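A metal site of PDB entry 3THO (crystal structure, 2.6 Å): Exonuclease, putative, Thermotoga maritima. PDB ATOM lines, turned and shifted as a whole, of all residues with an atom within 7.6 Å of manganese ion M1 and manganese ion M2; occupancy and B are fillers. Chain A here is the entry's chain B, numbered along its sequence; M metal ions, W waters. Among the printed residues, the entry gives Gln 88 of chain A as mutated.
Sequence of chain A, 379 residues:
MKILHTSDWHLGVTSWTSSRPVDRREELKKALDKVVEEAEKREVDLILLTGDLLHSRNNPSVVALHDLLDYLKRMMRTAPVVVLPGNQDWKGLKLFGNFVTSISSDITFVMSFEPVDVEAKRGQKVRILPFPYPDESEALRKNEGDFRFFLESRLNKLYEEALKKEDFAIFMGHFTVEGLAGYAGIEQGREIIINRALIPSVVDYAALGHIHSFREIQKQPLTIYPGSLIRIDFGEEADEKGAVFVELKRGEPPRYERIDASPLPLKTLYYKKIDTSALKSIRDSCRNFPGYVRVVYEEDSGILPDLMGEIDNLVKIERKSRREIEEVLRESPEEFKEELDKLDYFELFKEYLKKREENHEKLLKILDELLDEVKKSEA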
ATOM      1  N   SER A   7       1.688  24.717 -12.834  1.00  0.00           N
ATOM      2  CA  SER A   7       1.549  24.102 -11.523  1.00  0.00           C
ATOM      3  C   SER A   7       0.512  22.970 -11.551  1.00  0.00           C
ATOM      4  O   SER A   7      -0.219  22.808 -12.521  1.00  0.00           O
ATOM      5  CB  SER A   7       1.044  25.193 -10.544  1.00  0.00           C
ATOM      6  OG  SER A   7       1.158  24.815  -9.179  1.00  0.00           O
ATOM      7  N   ASP A   8       0.479  22.201 -10.460  1.00  0.00           N
ATOM      8  CA  ASP A   8      -0.579  21.243 -10.201  1.00  0.00           C
ATOM      9  C   ASP A   8      -0.791  20.177 -11.304  1.00  0.00           C
ATOM     10  O   ASP A   8      -1.899  19.671 -11.483  1.00  0.00           O
ATOM     11  CB  ASP A   8      -1.886  21.990  -9.858  1.00  0.00           C
ATOM     12  CG  ASP A   8      -1.737  22.854  -8.607  1.00  0.00           C
ATOM     13  OD1 ASP A   8      -1.243  24.023  -8.693  1.00  0.00           O
ATOM     14  OD2 ASP A   8      -2.117  22.373  -7.503  1.00  0.00           O
ATOM     15  N   TRP A   9       0.293  19.842 -11.988  1.00  0.00           N
ATOM     16  CA  TRP A   9       0.328  18.809 -13.009  1.00  0.00           C
ATOM     17  C   TRP A   9      -0.310  17.484 -12.554  1.00  0.00           C
ATOM     18  O   TRP A   9      -1.134  16.901 -13.263  1.00  0.00           O
ATOM     19  CB  TRP A   9       1.766  18.509 -13.420  1.00  0.00           C
ATOM     20  CG  TRP A   9       2.483  19.692 -13.980  1.00  0.00           C
ATOM     21  CD1 TRP A   9       1.976  20.938 -14.180  1.00  0.00           C
ATOM     22  CD2 TRP A   9       3.845  19.724 -14.458  1.00  0.00           C
ATOM     23  NE1 TRP A   9       2.930  21.762 -14.743  1.00  0.00           N
ATOM     24  CE2 TRP A   9       4.085  21.045 -14.907  1.00  0.00           C
ATOM     25  CE3 TRP A   9       4.879  18.777 -14.529  1.00  0.00           C
ATOM     26  CZ2 TRP A   9       5.327  21.435 -15.433  1.00  0.00           C
ATOM     27  CZ3 TRP A   9       6.108  19.168 -15.049  1.00  0.00           C
ATOM     28  CH2 TRP A   9       6.326  20.498 -15.498  1.00  0.00           C
ATOM     29  N   HIS A  10       0.120  16.990 -11.401  1.00  0.00           N
ATOM     30  CA  HIS A  10      -0.410  15.726 -10.874  1.00  0.00           C
ATOM     31  C   HIS A  10      -0.031  14.497 -11.735  1.00  0.00           C
ATOM     32  O   HIS A  10      -0.782  13.536 -11.799  1.00  0.00           O
ATOM     33  CB  HIS A  10      -1.925  15.811 -10.726  1.00  0.00           C
ATOM     34  CG  HIS A  10      -2.375  16.575  -9.520  1.00  0.00           C
ATOM     35  ND1 HIS A  10      -2.634  15.974  -8.306  1.00  0.00           N
ATOM     36  CD2 HIS A  10      -2.607  17.894  -9.329  1.00  0.00           C
ATOM     37  CE1 HIS A  10      -3.017  16.877  -7.426  1.00  0.00           C
ATOM     38  NE2 HIS A  10      -3.011  18.067  -8.030  1.00  0.00           N
ATOM     39  N   THR A  50       5.117  25.647  -9.407  1.00  0.00           N
ATOM     40  CA  THR A  50       4.730  25.848  -8.017  1.00  0.00           C
ATOM     41  C   THR A  50       4.049  24.659  -7.293  1.00  0.00           C
ATOM     42  O   THR A  50       3.180  24.873  -6.424  1.00  0.00           O
ATOM     43  CB  THR A  50       3.843  27.099  -7.868  1.00  0.00           C
ATOM     44  OG1 THR A  50       2.825  27.077  -8.873  1.00  0.00           O
ATOM     45  CG2 THR A  50       4.671  28.403  -8.012  1.00  0.00           C
ATOM     46  N   GLY A  51       4.406  23.429  -7.653  1.00  0.00           N
ATOM     47  CA  GLY A  51       4.101  22.272  -6.814  1.00  0.00           C
ATOM     48  C   GLY A  51       2.984  21.337  -7.267  1.00  0.00           C
ATOM     49  O   GLY A  51       2.206  21.673  -8.182  1.00  0.00           O
ATOM     50  N   ASP A  52       2.884  20.168  -6.616  1.00  0.00           N
ATOM     51  CA  ASP A  52       2.013  19.065  -7.044  1.00  0.00           C
ATOM     52  C   ASP A  52       2.230  18.711  -8.518  1.00  0.00           C
ATOM     53  O   ASP A  52       1.279  18.558  -9.280  1.00  0.00           O
ATOM     54  CB  ASP A  52       0.545  19.385  -6.791  1.00  0.00           C
ATOM     55  CG  ASP A  52       0.231  19.593  -5.327  1.00  0.00           C
ATOM     56  OD1 ASP A  52       1.041  19.168  -4.465  1.00  0.00           O
ATOM     57  OD2 ASP A  52      -0.837  20.160  -5.032  1.00  0.00           O
ATOM     58  N   LEU A  53       3.503  18.612  -8.899  1.00  0.00           N
ATOM     59  CA  LEU A  53       3.865  18.149 -10.232  1.00  0.00           C
ATOM     60  C   LEU A  53       3.648  16.632 -10.308  1.00  0.00           C
ATOM     61  O   LEU A  53       3.308  16.068 -11.358  1.00  0.00           O
ATOM     62  CB  LEU A  53       5.336  18.504 -10.523  1.00  0.00           C
ATOM     63  CG  LEU A  53       5.750  19.966 -10.363  1.00  0.00           C
ATOM     64  CD1 LEU A  53       7.203  20.165 -10.785  1.00  0.00           C
ATOM     65  CD2 LEU A  53       4.837  20.890 -11.186  1.00  0.00           C
ATOM     66  N   LEU A  54       3.856  15.963  -9.164  1.00  0.00           N
ATOM     67  CA  LEU A  54       3.528  14.553  -9.000  1.00  0.00           C
ATOM     68  C   LEU A  54       2.201  14.419  -8.288  1.00  0.00           C
ATOM     69  O   LEU A  54       1.757  15.341  -7.594  1.00  0.00           O
ATOM     70  CB  LEU A  54       4.597  13.848  -8.184  1.00  0.00           C
ATOM     71  CG  LEU A  54       5.912  13.773  -8.955  1.00  0.00           C
ATOM     72  CD1 LEU A  54       7.059  13.351  -8.033  1.00  0.00           C
ATOM     73  CD2 LEU A  54       5.756  12.820 -10.135  1.00  0.00           C
ATOM     74  N   HIS A  55       1.556  13.272  -8.454  1.00  0.00           N
ATOM     75  CA  HIS A  55       0.256  13.057  -7.838  1.00  0.00           C
ATOM     76  C   HIS A  55       0.357  12.433  -6.449  1.00  0.00           C
ATOM     77  O   HIS A  55      -0.443  12.750  -5.537  1.00  0.00           O
ATOM     78  CB  HIS A  55      -0.631  12.171  -8.728  1.00  0.00           C
ATOM     79  CG  HIS A  55      -1.979  11.940  -8.141  1.00  0.00           C
ATOM     80  ND1 HIS A  55      -2.895  12.951  -7.982  1.00  0.00           N
ATOM     81  CD2 HIS A  55      -2.543  10.829  -7.614  1.00  0.00           C
ATOM     82  CE1 HIS A  55      -3.989  12.466  -7.408  1.00  0.00           C
ATOM     83  NE2 HIS A  55      -3.802  11.179  -7.180  1.00  0.00           N
ATOM     84  N   PRO A  85       8.134  22.588  -4.442  1.00  0.00           N
ATOM     85  CA  PRO A  85       7.324  21.371  -4.239  1.00  0.00           C
ATOM     86  C   PRO A  85       6.054  21.617  -3.410  1.00  0.00           C
ATOM     87  O   PRO A  85       6.064  22.463  -2.516  1.00  0.00           O
ATOM     88  CB  PRO A  85       8.285  20.435  -3.475  1.00  0.00           C
ATOM     89  CG  PRO A  85       9.668  20.939  -3.851  1.00  0.00           C
ATOM     90  CD  PRO A  85       9.521  22.442  -3.967  1.00  0.00           C
ATOM     91  N   GLY A  86       4.988  20.882  -3.710  1.00  0.00           N
ATOM     92  CA  GLY A  86       3.732  20.989  -2.986  1.00  0.00           C
ATOM     93  C   GLY A  86       3.543  19.854  -2.006  1.00  0.00           C
ATOM     94  O   GLY A  86       4.390  18.947  -1.891  1.00  0.00           O
ATOM     95  N   ASN A  87       2.424  19.882  -1.277  1.00  0.00           N
ATOM     96  CA  ASN A  87       2.092  18.857  -0.292  1.00  0.00           C
ATOM     97  C   ASN A  87       1.922  17.455  -0.897  1.00  0.00           C
ATOM     98  O   ASN A  87       2.217  16.468  -0.261  1.00  0.00           O
ATOM     99  CB  ASN A  87       0.816  19.248   0.454  1.00  0.00           C
ATOM    100  CG  ASN A  87      -0.348  19.445  -0.488  1.00  0.00           C
ATOM    101  OD1 ASN A  87      -0.233  20.215  -1.452  1.00  0.00           O
ATOM    102  ND2 ASN A  87      -1.450  18.744  -0.260  1.00  0.00           N
ATOM    103  N   GLN A  88       1.435  17.381  -2.132  1.00  0.00           N
ATOM    104  CA  GLN A  88       1.268  16.081  -2.774  1.00  0.00           C
ATOM    105  C   GLN A  88       2.504  15.571  -3.519  1.00  0.00           C
ATOM    106  O   GLN A  88       2.515  14.435  -4.001  1.00  0.00           O
ATOM    107  CB  GLN A  88       0.088  16.119  -3.734  1.00  0.00           C
ATOM    108  CG  GLN A  88      -1.233  15.895  -3.049  1.00  0.00           C
ATOM    109  CD  GLN A  88      -2.375  16.482  -3.822  1.00  0.00           C
ATOM    110  OE1 GLN A  88      -3.138  15.748  -4.466  1.00  0.00           O
ATOM    111  NE2 GLN A  88      -2.525  17.820  -3.757  1.00  0.00           N
ATOM    112  N   ASP A  89       3.545  16.391  -3.649  1.00  0.00           N
ATOM    113  CA  ASP A  89       4.750  15.901  -4.322  1.00  0.00           C
ATOM    114  C   ASP A  89       5.441  14.861  -3.447  1.00  0.00           C
ATOM    115  O   ASP A  89       5.526  15.000  -2.233  1.00  0.00           O
ATOM    116  CB  ASP A  89       5.701  17.050  -4.683  1.00  0.00           C
ATOM    117  CG  ASP A  89       5.237  17.838  -5.934  1.00  0.00           C
ATOM    118  OD1 ASP A  89       4.862  17.202  -6.956  1.00  0.00           O
ATOM    119  OD2 ASP A  89       5.246  19.098  -5.898  1.00  0.00           O
ATOM    120  N   TYR A 133       3.937  24.770   1.459  1.00  0.00           N
ATOM    121  CA  TYR A 133       2.684  24.387   2.071  1.00  0.00           C
ATOM    122  C   TYR A 133       2.844  24.267   3.595  1.00  0.00           C
ATOM    123  O   TYR A 133       3.819  23.701   4.068  1.00  0.00           O
ATOM    124  CB  TYR A 133       2.245  23.048   1.487  1.00  0.00           C
ATOM    125  CG  TYR A 133       0.907  22.586   1.971  1.00  0.00           C
ATOM    126  CD1 TYR A 133      -0.254  23.082   1.390  1.00  0.00           C
ATOM    127  CD2 TYR A 133       0.795  21.647   3.000  1.00  0.00           C
ATOM    128  CE1 TYR A 133      -1.510  22.661   1.802  1.00  0.00           C
ATOM    129  CE2 TYR A 133      -0.447  21.221   3.428  1.00  0.00           C
ATOM    130  CZ  TYR A 133      -1.604  21.727   2.821  1.00  0.00           C
ATOM    131  OH  TYR A 133      -2.854  21.312   3.229  1.00  0.00           O
ATOM    132  N   HIS A 174       2.667  27.843  -1.987  1.00  0.00           N
ATOM    133  CA  HIS A 174       1.809  26.674  -2.231  1.00  0.00           C
ATOM    134  C   HIS A 174       0.881  26.489  -1.043  1.00  0.00           C
ATOM    135  O   HIS A 174       1.291  25.949  -0.010  1.00  0.00           O
ATOM    136  CB  HIS A 174       2.634  25.418  -2.484  1.00  0.00           C
ATOM    137  CG  HIS A 174       1.842  24.264  -3.027  1.00  0.00           C
ATOM    138  ND1 HIS A 174       1.784  23.948  -4.359  1.00  0.00           N
ATOM    139  CD2 HIS A 174       1.054  23.363  -2.384  1.00  0.00           C
ATOM    140  CE1 HIS A 174       1.003  22.893  -4.533  1.00  0.00           C
ATOM    141  NE2 HIS A 174       0.554  22.520  -3.359  1.00  0.00           N
ATOM    142  N   PHE A 175      -0.356  26.954  -1.204  1.00  0.00           N
ATOM    143  CA  PHE A 175      -1.359  26.986  -0.126  1.00  0.00           C
ATOM    144  C   PHE A 175      -2.682  27.550  -0.652  1.00  0.00           C
ATOM    145  O   PHE A 175      -2.784  28.000  -1.826  1.00  0.00           O
ATOM    146  CB  PHE A 175      -0.886  27.841   1.056  1.00  0.00           C
ATOM    147  CG  PHE A 175      -0.498  29.233   0.657  1.00  0.00           C
ATOM    148  CD1 PHE A 175      -1.455  30.221   0.557  1.00  0.00           C
ATOM    149  CD2 PHE A 175       0.823  29.549   0.337  1.00  0.00           C
ATOM    150  CE1 PHE A 175      -1.105  31.521   0.155  1.00  0.00           C
ATOM    151  CE2 PHE A 175       1.191  30.849  -0.063  1.00  0.00           C
ATOM    152  CZ  PHE A 175       0.215  31.832  -0.153  1.00  0.00           C
ATOM    153  N   THR A 176      -3.686  27.527   0.205  1.00  0.00           N
ATOM    154  CA  THR A 176      -5.033  27.985  -0.137  1.00  0.00           C
ATOM    155  C   THR A 176      -5.237  29.388   0.428  1.00  0.00           C
ATOM    156  O   THR A 176      -5.018  29.594   1.620  1.00  0.00           O
ATOM    157  CB  THR A 176      -6.065  27.061   0.537  1.00  0.00           C
ATOM    158  OG1 THR A 176      -5.897  25.704   0.077  1.00  0.00           O
ATOM    159  CG2 THR A 176      -7.502  27.549   0.308  1.00  0.00           C
ATOM    160  N   GLU A 191      -6.978  22.616   6.475  1.00  0.00           N
ATOM    161  CA  GLU A 191      -5.796  23.341   6.008  1.00  0.00           C
ATOM    162  C   GLU A 191      -5.635  24.616   6.816  1.00  0.00           C
ATOM    163  O   GLU A 191      -6.609  25.150   7.349  1.00  0.00           O
ATOM    164  CB  GLU A 191      -5.929  23.724   4.528  1.00  0.00           C
ATOM    165  CG  GLU A 191      -5.700  22.602   3.517  1.00  0.00           C
ATOM    166  CD  GLU A 191      -5.601  23.143   2.088  1.00  0.00           C
ATOM    167  OE1 GLU A 191      -5.253  24.338   1.928  1.00  0.00           O
ATOM    168  OE2 GLU A 191      -5.860  22.387   1.121  1.00  0.00           O
ATOM    169  N   GLY A 209       0.481  27.802  -6.322  1.00  0.00           N
ATOM    170  CA  GLY A 209      -0.005  26.503  -6.760  1.00  0.00           C
ATOM    171  C   GLY A 209      -0.841  25.871  -5.645  1.00  0.00           C
ATOM    172  O   GLY A 209      -0.874  26.418  -4.520  1.00  0.00           O
ATOM    173  N   HIS A 210      -1.503  24.747  -5.942  1.00  0.00           N
ATOM    174  CA  HIS A 210      -2.273  23.924  -4.976  1.00  0.00           C
ATOM    175  C   HIS A 210      -3.772  23.888  -5.324  1.00  0.00           C
ATOM    176  O   HIS A 210      -4.495  22.957  -4.951  1.00  0.00           O
ATOM    177  CB  HIS A 210      -2.065  24.380  -3.513  1.00  0.00           C
ATOM    178  CG  HIS A 210      -2.795  23.547  -2.498  1.00  0.00           C
ATOM    179  ND1 HIS A 210      -2.529  22.227  -2.263  1.00  0.00           N
ATOM    180  CD2 HIS A 210      -3.829  23.879  -1.669  1.00  0.00           C
ATOM    181  CE1 HIS A 210      -3.335  21.754  -1.320  1.00  0.00           C
ATOM    182  NE2 HIS A 210      -4.129  22.732  -0.948  1.00  0.00           N
ATOM    183  N   ILE A 211      -4.216  24.906  -6.054  1.00  0.00           N
ATOM    184  CA  ILE A 211      -5.619  25.118  -6.438  1.00  0.00           C
ATOM    185  C   ILE A 211      -5.728  24.836  -7.941  1.00  0.00           C
ATOM    186  O   ILE A 211      -4.870  25.267  -8.724  1.00  0.00           O
ATOM    187  CB  ILE A 211      -6.028  26.584  -6.148  1.00  0.00           C
ATOM    188  CG1 ILE A 211      -6.054  26.853  -4.640  1.00  0.00           C
ATOM    189  CG2 ILE A 211      -7.363  26.926  -6.778  1.00  0.00           C
ATOM    190  CD1 ILE A 211      -7.204  26.246  -3.954  1.00  0.00           C
ATOM    191  N   HIS A 212      -6.768  24.112  -8.348  1.00  0.00           N
ATOM    192  CA  HIS A 212      -6.786  23.539  -9.704  1.00  0.00           C
ATOM    193  C   HIS A 212      -7.439  24.432 -10.730  1.00  0.00           C
ATOM    194  O   HIS A 212      -7.265  24.229 -11.938  1.00  0.00           O
ATOM    195  CB  HIS A 212      -7.444  22.150  -9.720  1.00  0.00           C
ATOM    196  CG  HIS A 212      -6.819  21.155  -8.770  1.00  0.00           C
ATOM    197  ND1 HIS A 212      -7.388  19.956  -8.492  1.00  0.00           N
ATOM    198  CD2 HIS A 212      -5.666  21.240  -8.049  1.00  0.00           C
ATOM    199  CE1 HIS A 212      -6.623  19.291  -7.622  1.00  0.00           C
ATOM    200  NE2 HIS A 212      -5.575  20.045  -7.349  1.00  0.00           N
ATOM    201  N   SER A 228      -4.728  23.524 -12.690  1.00  0.00           N
ATOM    202  CA  SER A 228      -4.222  22.291 -13.288  1.00  0.00           C
ATOM    203  C   SER A 228      -4.227  22.314 -14.827  1.00  0.00           C
ATOM    204  O   SER A 228      -4.677  23.270 -15.444  1.00  0.00           O
ATOM    205  CB  SER A 228      -4.986  21.089 -12.735  1.00  0.00           C
ATOM    206  OG  SER A 228      -6.375  21.285 -12.839  1.00  0.00           O
ATOM    207  N   ILE A 232      -9.562  17.212 -13.119  1.00  0.00           N
ATOM    208  CA  ILE A 232      -9.186  16.073 -12.315  1.00  0.00           C
ATOM    209  C   ILE A 232     -10.420  15.327 -11.818  1.00  0.00           C
ATOM    210  O   ILE A 232     -10.411  14.095 -11.764  1.00  0.00           O
ATOM    211  CB  ILE A 232      -8.192  16.502 -11.187  1.00  0.00           C
ATOM    212  CG1 ILE A 232      -6.936  17.115 -11.840  1.00  0.00           C
ATOM    213  CG2 ILE A 232      -7.827  15.333 -10.305  1.00  0.00           C
ATOM    214  CD1 ILE A 232      -5.696  17.118 -11.008  1.00  0.00           C
HETATM  215 MN    MN M   1      -1.172  21.226  -3.171  1.00  0.00          MN
HETATM  216 MN    MN M   2      -2.977  20.208  -6.303  1.00  0.00          MN
HETATM  217  O   HOH W   1      -5.182  20.712  -4.015  1.00  0.00           O
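Merely in contact with manganese ion M2: Gln 88 (3.5 Å).
Six residues have an atom within 4 Å of manganese ion M2: Asp 8, His 10, Asp 52, Gln 88, His 210 and His 212.
The nearest printed residue that does not touch manganese ion M2 is Ile 211 (4.9 Å).
Manganese ion M1 is bound by a ring nitrogen (ND1) of His 210 (1.9 Å), a ring nitrogen (NE2) of His 174 (2.2 Å), the side-chain carboxylate of Asp 52 (2.2 Å) and the side-chain amide oxygen of Asn 87 (2.2 Å).
Manganese ion M1 has four donor atoms within binding distance.
Water W1 bridges O of His 210 and NE2 of His 212.
Merely in contact with manganese ion M1: Gln 88 (3.7 Å).
Of the 26 residues printed, 5 come within 4 Å of manganese ion M1.
The nearest printed residue that does not touch manganese ion M1 is Asp 8 (4.6 Å).
OD1 of Asp 8 lies within hydrogen-bond range of OG of Ser 7 (2.6 Å).
The backbone NH (N) of Asp 52 lies within hydrogen-bond range of the side-chain carboxylate (OD2) of Asp 89.
ND1 of His 174 lies within hydrogen-bond range of O of Thr 50.
O of Asp 52 sits at hydrogen-bond distance from N of His 10.
The side-chain carboxylate (OD1) of Asp 8 lies within hydrogen-bond range of the backbone NH (N) of His 210 (2.9 Å).
The backbone carbonyl oxygen (O) of Leu 53 is in hydrogen-bond range of the backbone NH (N) of His 10 (3.3 Å).
The side-chain carboxylate of Glu 191 lies within hydrogen-bond range of a ring nitrogen (NE2) of His 210.
OD1 of Asp 52 sits at hydrogen-bond distance from N of Gln 88 (3.0 Å).
Manganese ion M2 is bound by OD2 of Asp 52 (2.5 Å) and OD2 of Asp 8 (2.6 Å).
Manganese ion M2 has two donor atoms within binding distance.
Slightly farther from manganese ion M2 lies a ring nitrogen (NE2) of His 10 (2.8 Å).
Slightly farther from manganese ion M2 lies NE2 of His 212 (2.8 Å).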
